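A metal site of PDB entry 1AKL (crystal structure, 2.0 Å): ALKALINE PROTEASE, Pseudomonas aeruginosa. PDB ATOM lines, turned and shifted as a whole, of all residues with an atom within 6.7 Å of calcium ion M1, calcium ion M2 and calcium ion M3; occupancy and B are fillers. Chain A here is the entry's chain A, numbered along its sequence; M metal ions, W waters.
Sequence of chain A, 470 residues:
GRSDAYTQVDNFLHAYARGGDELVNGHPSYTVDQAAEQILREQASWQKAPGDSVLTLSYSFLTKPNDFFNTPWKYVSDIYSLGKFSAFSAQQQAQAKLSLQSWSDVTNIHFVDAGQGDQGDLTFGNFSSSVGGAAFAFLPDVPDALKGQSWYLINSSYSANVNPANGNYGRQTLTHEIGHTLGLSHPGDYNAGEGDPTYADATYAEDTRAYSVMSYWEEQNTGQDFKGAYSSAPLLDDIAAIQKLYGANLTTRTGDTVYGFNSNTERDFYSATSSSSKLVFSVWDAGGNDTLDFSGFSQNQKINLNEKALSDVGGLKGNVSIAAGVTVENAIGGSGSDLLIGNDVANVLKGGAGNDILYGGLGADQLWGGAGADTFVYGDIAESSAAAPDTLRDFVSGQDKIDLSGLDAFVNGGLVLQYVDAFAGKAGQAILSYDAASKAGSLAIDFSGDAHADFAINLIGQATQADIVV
Within 4 Å of calcium ion M1: Gly 370, Ala 371, Gly 372, Asp 374, Gln 399 and Asp 400. The nearest printed residue that does not touch calcium ion M1 is Ala 373 (4.5 Å).
OD1 of Asp 338 sits at hydrogen-bond distance from N of Gln 301. OD2 of Asp 394 sits at hydrogen-bond distance from N of Gly 370. The side-chain amide nitrogen (NE2) of Gln 301 lies close to the backbone NH (N) of Gly 334, at 3.5 Å. N of Gly 369 sits at hydrogen-bond distance from OD1 of Asp 394 (3.0 Å). O of Trp 368 sits at hydrogen-bond distance from N of Gly 351, at 2.9 Å. The backbone NH (N) of Val 396 lies within hydrogen-bond range of the side-chain carboxylate (OD2) of Asp 400, at 3.1 Å.
Calcium ion M2 is bound by the backbone carbonyl oxygen (O) of Gly 369, the backbone carbonyl oxygen (O) of Ala 371, the backbone carbonyl oxygen (O) of Gly 352, the backbone carbonyl oxygen (O) of Gly 354, the side-chain carboxylate (OD1) of Asp 374 and the side-chain carboxylate (OD2) of Asp 356. Calcium ion M2 has six donor atoms within binding distance. Slightly farther from calcium ion M2 lies the side-chain carboxylate (OD2) of Asp 374 (3.1 Å).
Within 4 Å of calcium ion M2: Gly 352, Ala 353, Gly 354, Asp 356, Gly 369, Gly 370, Ala 371 and Asp 374. The nearest printed residue that does not touch calcium ion M2 is Gly 351 (4.2 Å).
Calcium ion M3 is bound by the backbone carbonyl oxygen (O) of Gly 334 (2.2 Å), the backbone carbonyl oxygen (O) of Gly 336 (2.2 Å), the backbone carbonyl oxygen (O) of Ala 353 (2.3 Å), the backbone carbonyl oxygen (O) of Gly 351 (2.3 Å), the side-chain carboxylate (OD1) of Asp 356 (2.5 Å) and the side-chain carboxylate (OD2) of Asp 338 (2.7 Å).
Water W1 lies within hydrogen-bond range of the side-chain carboxylate of Asp 400 (2.6 Å) and the backbone carbonyl oxygen of Asp 394 (3.2 Å).
Ser 335 touches calcium ion M3 (C to CA, 3.9 Å). Eight residues have an atom within 4 Å of calcium ion M3: Gly 334, Ser 335, Gly 336, Asp 338, Gly 351, Gly 352, Ala 353 and Asp 356.
Calcium ion M1 is bound by the backbone carbonyl oxygen of Gly 372 (2.2 Å), water W1 (2.4 Å), the backbone carbonyl oxygen of Gly 370 (2.5 Å), the side-chain carboxylate of Asp 400 (2.7 Å), the side-chain carboxylate of Asp 374 (2.8 Å) and the side-chain amide oxygen of Gln 399 (2.8 Å).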
ATOM      1  N   GLN A 299      18.573 -17.934 -17.054  1.00  0.00           N
ATOM      2  CA  GLN A 299      19.617 -17.485 -16.142  1.00  0.00           C
ATOM      3  C   GLN A 299      19.085 -16.546 -15.084  1.00  0.00           C
ATOM      4  O   GLN A 299      18.002 -15.979 -15.228  1.00  0.00           O
ATOM      5  CB  GLN A 299      20.715 -16.756 -16.907  1.00  0.00           C
ATOM      6  CG  GLN A 299      21.432 -17.588 -17.913  1.00  0.00           C
ATOM      7  CD  GLN A 299      20.788 -17.552 -19.250  1.00  0.00           C
ATOM      8  OE1 GLN A 299      19.625 -17.196 -19.390  1.00  0.00           O
ATOM      9  NE2 GLN A 299      21.545 -17.914 -20.264  1.00  0.00           N
ATOM     10  N   GLN A 301      18.772 -13.200 -13.530  1.00  0.00           N
ATOM     11  CA  GLN A 301      18.922 -11.867 -14.095  1.00  0.00           C
ATOM     12  C   GLN A 301      18.678 -10.762 -13.083  1.00  0.00           C
ATOM     13  O   GLN A 301      18.042 -10.994 -12.063  1.00  0.00           O
ATOM     14  CB  GLN A 301      17.925 -11.712 -15.240  1.00  0.00           C
ATOM     15  CG  GLN A 301      17.891 -12.898 -16.174  1.00  0.00           C
ATOM     16  CD  GLN A 301      16.910 -12.689 -17.306  1.00  0.00           C
ATOM     17  OE1 GLN A 301      17.219 -11.977 -18.270  1.00  0.00           O
ATOM     18  NE2 GLN A 301      15.742 -13.276 -17.206  1.00  0.00           N
ATOM     19  N   GLY A 333      10.629 -11.009 -15.684  1.00  0.00           N
ATOM     20  CA  GLY A 333      11.792 -11.846 -15.501  1.00  0.00           C
ATOM     21  C   GLY A 333      11.559 -13.213 -16.098  1.00  0.00           C
ATOM     22  O   GLY A 333      10.466 -13.493 -16.594  1.00  0.00           O
ATOM     23  N   GLY A 334      12.565 -14.072 -16.039  1.00  0.00           N
ATOM     24  CA  GLY A 334      12.448 -15.419 -16.575  1.00  0.00           C
ATOM     25  C   GLY A 334      12.323 -16.459 -15.478  1.00  0.00           C
ATOM     26  O   GLY A 334      12.071 -16.128 -14.327  1.00  0.00           O
ATOM     27  N   SER A 335      12.584 -17.720 -15.805  1.00  0.00           N
ATOM     28  CA  SER A 335      12.468 -18.783 -14.821  1.00  0.00           C
ATOM     29  C   SER A 335      13.585 -18.858 -13.786  1.00  0.00           C
ATOM     30  O   SER A 335      13.525 -19.659 -12.854  1.00  0.00           O
ATOM     31  CB  SER A 335      12.281 -20.128 -15.524  1.00  0.00           C
ATOM     32  OG  SER A 335      13.328 -20.386 -16.433  1.00  0.00           O
ATOM     33  N   GLY A 336      14.604 -18.009 -13.933  1.00  0.00           N
ATOM     34  CA  GLY A 336      15.687 -18.016 -12.970  1.00  0.00           C
ATOM     35  C   GLY A 336      15.285 -17.140 -11.797  1.00  0.00           C
ATOM     36  O   GLY A 336      14.223 -16.497 -11.831  1.00  0.00           O
ATOM     37  N   SER A 337      16.096 -17.136 -10.754  1.00  0.00           N
ATOM     38  CA  SER A 337      15.818 -16.308  -9.589  1.00  0.00           C
ATOM     39  C   SER A 337      16.336 -14.916  -9.914  1.00  0.00           C
ATOM     40  O   SER A 337      17.543 -14.682  -9.955  1.00  0.00           O
ATOM     41  CB  SER A 337      16.487 -16.891  -8.345  1.00  0.00           C
ATOM     42  OG  SER A 337      15.885 -18.136  -7.993  1.00  0.00           O
ATOM     43  N   ASP A 338      15.410 -13.991 -10.158  1.00  0.00           N
ATOM     44  CA  ASP A 338      15.740 -12.629 -10.567  1.00  0.00           C
ATOM     45  C   ASP A 338      15.616 -11.555  -9.501  1.00  0.00           C
ATOM     46  O   ASP A 338      15.001 -11.751  -8.451  1.00  0.00           O
ATOM     47  CB  ASP A 338      14.858 -12.222 -11.738  1.00  0.00           C
ATOM     48  CG  ASP A 338      14.761 -13.289 -12.798  1.00  0.00           C
ATOM     49  OD1 ASP A 338      15.789 -13.929 -13.113  1.00  0.00           O
ATOM     50  OD2 ASP A 338      13.639 -13.502 -13.308  1.00  0.00           O
ATOM     51  N   LEU A 340      14.278  -7.668  -9.621  1.00  0.00           N
ATOM     52  CA  LEU A 340      13.663  -6.651 -10.447  1.00  0.00           C
ATOM     53  C   LEU A 340      13.448  -5.381  -9.681  1.00  0.00           C
ATOM     54  O   LEU A 340      12.677  -5.364  -8.735  1.00  0.00           O
ATOM     55  CB  LEU A 340      12.323  -7.136 -10.993  1.00  0.00           C
ATOM     56  CG  LEU A 340      12.249  -8.276 -12.016  1.00  0.00           C
ATOM     57  CD1 LEU A 340      12.309  -9.611 -11.321  1.00  0.00           C
ATOM     58  CD2 LEU A 340      10.949  -8.166 -12.787  1.00  0.00           C
ATOM     59  N   LYS A 350       7.042  -8.585 -12.990  1.00  0.00           N
ATOM     60  CA  LYS A 350       6.640  -9.977 -12.923  1.00  0.00           C
ATOM     61  C   LYS A 350       7.878 -10.835 -12.807  1.00  0.00           C
ATOM     62  O   LYS A 350       8.684 -10.885 -13.722  1.00  0.00           O
ATOM     63  CB  LYS A 350       5.831 -10.369 -14.150  1.00  0.00           C
ATOM     64  CG  LYS A 350       4.512  -9.632 -14.267  1.00  0.00           C
ATOM     65  CD  LYS A 350       3.699 -10.148 -15.427  1.00  0.00           C
ATOM     66  CE  LYS A 350       2.297  -9.566 -15.425  1.00  0.00           C
ATOM     67  NZ  LYS A 350       1.519  -9.974 -16.638  1.00  0.00           N
ATOM     68  N   GLY A 351       8.034 -11.518 -11.689  1.00  0.00           N
ATOM     69  CA  GLY A 351       9.215 -12.323 -11.505  1.00  0.00           C
ATOM     70  C   GLY A 351       9.241 -13.655 -12.209  1.00  0.00           C
ATOM     71  O   GLY A 351      10.315 -14.258 -12.338  1.00  0.00           O
ATOM     72  N   GLY A 352       8.069 -14.144 -12.607  1.00  0.00           N
ATOM     73  CA  GLY A 352       8.001 -15.431 -13.275  1.00  0.00           C
ATOM     74  C   GLY A 352       8.434 -16.521 -12.314  1.00  0.00           C
ATOM     75  O   GLY A 352       8.460 -16.304 -11.101  1.00  0.00           O
ATOM     76  N   ALA A 353       8.807 -17.691 -12.825  1.00  0.00           N
ATOM     77  CA  ALA A 353       9.240 -18.772 -11.957  1.00  0.00           C
ATOM     78  C   ALA A 353      10.512 -18.380 -11.202  1.00  0.00           C
ATOM     79  O   ALA A 353      11.046 -17.288 -11.423  1.00  0.00           O
ATOM     80  CB  ALA A 353       9.467 -20.045 -12.753  1.00  0.00           C
ATOM     81  N   GLY A 354      10.981 -19.243 -10.323  1.00  0.00           N
ATOM     82  CA  GLY A 354      12.156 -18.929  -9.544  1.00  0.00           C
ATOM     83  C   GLY A 354      11.833 -18.006  -8.381  1.00  0.00           C
ATOM     84  O   GLY A 354      10.774 -17.343  -8.347  1.00  0.00           O
ATOM     85  N   ASN A 355      12.777 -17.920  -7.451  1.00  0.00           N
ATOM     86  CA  ASN A 355      12.615 -17.088  -6.265  1.00  0.00           C
ATOM     87  C   ASN A 355      13.161 -15.691  -6.499  1.00  0.00           C
ATOM     88  O   ASN A 355      14.356 -15.440  -6.391  1.00  0.00           O
ATOM     89  CB  ASN A 355      13.309 -17.756  -5.075  1.00  0.00           C
ATOM     90  CG  ASN A 355      12.688 -19.106  -4.736  1.00  0.00           C
ATOM     91  OD1 ASN A 355      11.568 -19.420  -5.161  1.00  0.00           O
ATOM     92  ND2 ASN A 355      13.413 -19.917  -3.980  1.00  0.00           N
ATOM     93  N   ASP A 356      12.253 -14.769  -6.780  1.00  0.00           N
ATOM     94  CA  ASP A 356      12.603 -13.395  -7.105  1.00  0.00           C
ATOM     95  C   ASP A 356      12.506 -12.401  -5.974  1.00  0.00           C
ATOM     96  O   ASP A 356      11.793 -12.605  -4.995  1.00  0.00           O
ATOM     97  CB  ASP A 356      11.729 -12.913  -8.259  1.00  0.00           C
ATOM     98  CG  ASP A 356      11.558 -13.959  -9.331  1.00  0.00           C
ATOM     99  OD1 ASP A 356      12.544 -14.296 -10.012  1.00  0.00           O
ATOM    100  OD2 ASP A 356      10.432 -14.453  -9.489  1.00  0.00           O
ATOM    101  N   LEU A 358      11.488  -8.535  -5.653  1.00  0.00           N
ATOM    102  CA  LEU A 358      10.838  -7.424  -6.339  1.00  0.00           C
ATOM    103  C   LEU A 358      10.900  -6.154  -5.490  1.00  0.00           C
ATOM    104  O   LEU A 358      10.533  -6.167  -4.322  1.00  0.00           O
ATOM    105  CB  LEU A 358       9.360  -7.746  -6.613  1.00  0.00           C
ATOM    106  CG  LEU A 358       8.859  -8.947  -7.437  1.00  0.00           C
ATOM    107  CD1 LEU A 358       8.965  -8.665  -8.896  1.00  0.00           C
ATOM    108  CD2 LEU A 358       9.539 -10.235  -7.050  1.00  0.00           C
ATOM    109  N   TRP A 368       3.997  -8.908  -9.157  1.00  0.00           N
ATOM    110  CA  TRP A 368       3.613 -10.308  -9.326  1.00  0.00           C
ATOM    111  C   TRP A 368       4.882 -11.121  -9.118  1.00  0.00           C
ATOM    112  O   TRP A 368       5.833 -10.992  -9.858  1.00  0.00           O
ATOM    113  CB  TRP A 368       3.100 -10.581 -10.738  1.00  0.00           C
ATOM    114  CG  TRP A 368       1.934  -9.780 -11.201  1.00  0.00           C
ATOM    115  CD1 TRP A 368       1.925  -8.441 -11.507  1.00  0.00           C
ATOM    116  CD2 TRP A 368       0.622 -10.267 -11.470  1.00  0.00           C
ATOM    117  NE1 TRP A 368       0.673  -8.074 -11.964  1.00  0.00           N
ATOM    118  CE2 TRP A 368      -0.139  -9.171 -11.947  1.00  0.00           C
ATOM    119  CE3 TRP A 368       0.011 -11.523 -11.351  1.00  0.00           C
ATOM    120  CZ2 TRP A 368      -1.479  -9.297 -12.305  1.00  0.00           C
ATOM    121  CZ3 TRP A 368      -1.329 -11.649 -11.709  1.00  0.00           C
ATOM    122  CH2 TRP A 368      -2.056 -10.529 -12.184  1.00  0.00           C
ATOM    123  N   GLY A 369       4.898 -11.986  -8.118  1.00  0.00           N
ATOM    124  CA  GLY A 369       6.087 -12.775  -7.900  1.00  0.00           C
ATOM    125  C   GLY A 369       6.100 -14.052  -8.710  1.00  0.00           C
ATOM    126  O   GLY A 369       7.169 -14.630  -8.964  1.00  0.00           O
ATOM    127  N   GLY A 370       4.921 -14.527  -9.075  1.00  0.00           N
ATOM    128  CA  GLY A 370       4.821 -15.767  -9.826  1.00  0.00           C
ATOM    129  C   GLY A 370       5.193 -16.967  -8.967  1.00  0.00           C
ATOM    130  O   GLY A 370       5.311 -16.870  -7.737  1.00  0.00           O
ATOM    131  N   ALA A 371       5.417 -18.101  -9.624  1.00  0.00           N
ATOM    132  CA  ALA A 371       5.793 -19.334  -8.947  1.00  0.00           C
ATOM    133  C   ALA A 371       7.016 -19.083  -8.069  1.00  0.00           C
ATOM    134  O   ALA A 371       7.754 -18.112  -8.294  1.00  0.00           O
ATOM    135  CB  ALA A 371       6.097 -20.404  -9.974  1.00  0.00           C
ATOM    136  N   GLY A 372       7.215 -19.917  -7.056  1.00  0.00           N
ATOM    137  CA  GLY A 372       8.364 -19.776  -6.174  1.00  0.00           C
ATOM    138  C   GLY A 372       8.181 -18.827  -5.010  1.00  0.00           C
ATOM    139  O   GLY A 372       7.222 -18.023  -4.986  1.00  0.00           O
ATOM    140  N   ALA A 373       9.111 -18.884  -4.073  1.00  0.00           N
ATOM    141  CA  ALA A 373       9.106 -18.055  -2.882  1.00  0.00           C
ATOM    142  C   ALA A 373       9.765 -16.731  -3.228  1.00  0.00           C
ATOM    143  O   ALA A 373      10.975 -16.645  -3.314  1.00  0.00           O
ATOM    144  CB  ALA A 373       9.874 -18.735  -1.774  1.00  0.00           C
ATOM    145  N   ASP A 374       8.943 -15.701  -3.371  1.00  0.00           N
ATOM    146  CA  ASP A 374       9.444 -14.389  -3.748  1.00  0.00           C
ATOM    147  C   ASP A 374       9.400 -13.416  -2.595  1.00  0.00           C
ATOM    148  O   ASP A 374       8.545 -13.548  -1.717  1.00  0.00           O
ATOM    149  CB  ASP A 374       8.600 -13.844  -4.905  1.00  0.00           C
ATOM    150  CG  ASP A 374       8.424 -14.862  -5.995  1.00  0.00           C
ATOM    151  OD1 ASP A 374       9.437 -15.314  -6.569  1.00  0.00           O
ATOM    152  OD2 ASP A 374       7.269 -15.257  -6.235  1.00  0.00           O
ATOM    153  N   PHE A 376       9.197  -9.324  -1.476  1.00  0.00           N
ATOM    154  CA  PHE A 376       8.807  -8.005  -1.942  1.00  0.00           C
ATOM    155  C   PHE A 376       9.445  -7.005  -0.978  1.00  0.00           C
ATOM    156  O   PHE A 376       9.002  -6.847   0.158  1.00  0.00           O
ATOM    157  CB  PHE A 376       7.283  -7.887  -1.978  1.00  0.00           C
ATOM    158  CG  PHE A 376       6.608  -8.972  -2.785  1.00  0.00           C
ATOM    159  CD1 PHE A 376       6.284 -10.190  -2.203  1.00  0.00           C
ATOM    160  CD2 PHE A 376       6.354  -8.796  -4.144  1.00  0.00           C
ATOM    161  CE1 PHE A 376       5.714 -11.217  -2.960  1.00  0.00           C
ATOM    162  CE2 PHE A 376       5.797  -9.812  -4.903  1.00  0.00           C
ATOM    163  CZ  PHE A 376       5.474 -11.028  -4.307  1.00  0.00           C
ATOM    164  N   ASP A 394      -0.495 -11.465  -6.303  1.00  0.00           N
ATOM    165  CA  ASP A 394      -0.483 -12.932  -6.216  1.00  0.00           C
ATOM    166  C   ASP A 394       0.285 -13.458  -5.007  1.00  0.00           C
ATOM    167  O   ASP A 394       1.094 -14.400  -5.118  1.00  0.00           O
ATOM    168  CB  ASP A 394       0.097 -13.521  -7.510  1.00  0.00           C
ATOM    169  CG  ASP A 394       1.573 -13.226  -7.690  1.00  0.00           C
ATOM    170  OD1 ASP A 394       2.140 -12.392  -6.943  1.00  0.00           O
ATOM    171  OD2 ASP A 394       2.172 -13.853  -8.580  1.00  0.00           O
ATOM    172  N   PHE A 395       0.020 -12.844  -3.850  1.00  0.00           N
ATOM    173  CA  PHE A 395       0.704 -13.225  -2.627  1.00  0.00           C
ATOM    174  C   PHE A 395       0.274 -14.608  -2.145  1.00  0.00           C
ATOM    175  O   PHE A 395      -0.879 -15.022  -2.290  1.00  0.00           O
ATOM    176  CB  PHE A 395       0.462 -12.171  -1.544  1.00  0.00           C
ATOM    177  CG  PHE A 395       1.467 -12.208  -0.437  1.00  0.00           C
ATOM    178  CD1 PHE A 395       2.690 -11.549  -0.571  1.00  0.00           C
ATOM    179  CD2 PHE A 395       1.217 -12.917   0.738  1.00  0.00           C
ATOM    180  CE1 PHE A 395       3.639 -11.582   0.461  1.00  0.00           C
ATOM    181  CE2 PHE A 395       2.159 -12.962   1.765  1.00  0.00           C
ATOM    182  CZ  PHE A 395       3.367 -12.294   1.630  1.00  0.00           C
ATOM    183  N   VAL A 396       1.233 -15.328  -1.587  1.00  0.00           N
ATOM    184  CA  VAL A 396       1.001 -16.667  -1.080  1.00  0.00           C
ATOM    185  C   VAL A 396       1.646 -16.772   0.273  1.00  0.00           C
ATOM    186  O   VAL A 396       2.867 -16.932   0.391  1.00  0.00           O
ATOM    187  CB  VAL A 396       1.623 -17.712  -2.016  1.00  0.00           C
ATOM    188  CG1 VAL A 396       1.712 -19.064  -1.320  1.00  0.00           C
ATOM    189  CG2 VAL A 396       0.791 -17.817  -3.272  1.00  0.00           C
ATOM    190  N   GLN A 399       4.944 -18.645   1.777  1.00  0.00           N
ATOM    191  CA  GLN A 399       5.820 -18.859   0.636  1.00  0.00           C
ATOM    192  C   GLN A 399       6.485 -17.524   0.296  1.00  0.00           C
ATOM    193  O   GLN A 399       7.703 -17.436   0.216  1.00  0.00           O
ATOM    194  CB  GLN A 399       5.033 -19.388  -0.567  1.00  0.00           C
ATOM    195  CG  GLN A 399       5.920 -19.923  -1.687  1.00  0.00           C
ATOM    196  CD  GLN A 399       5.146 -20.208  -2.980  1.00  0.00           C
ATOM    197  OE1 GLN A 399       4.794 -19.277  -3.733  1.00  0.00           O
ATOM    198  NE2 GLN A 399       4.920 -21.485  -3.268  1.00  0.00           N
ATOM    199  N   ASP A 400       5.675 -16.487   0.123  1.00  0.00           N
ATOM    200  CA  ASP A 400       6.171 -15.157  -0.192  1.00  0.00           C
ATOM    201  C   ASP A 400       6.383 -14.363   1.097  1.00  0.00           C
ATOM    202  O   ASP A 400       5.721 -14.619   2.108  1.00  0.00           O
ATOM    203  CB  ASP A 400       5.164 -14.401  -1.074  1.00  0.00           C
ATOM    204  CG  ASP A 400       4.871 -15.115  -2.383  1.00  0.00           C
ATOM    205  OD1 ASP A 400       5.596 -16.060  -2.767  1.00  0.00           O
ATOM    206  OD2 ASP A 400       3.899 -14.692  -3.037  1.00  0.00           O
HETATM  207 CA    CA M   1       5.294 -16.936  -5.276  1.00  0.00          CA
HETATM  208 CA    CA M   2       8.764 -16.122  -8.793  1.00  0.00          CA
HETATM  209 CA    CA M   3      12.260 -15.496 -12.215  1.00  0.00          CA
HETATM  210  O   HOH W   1       4.220 -14.818  -5.584  1.00  0.00           O
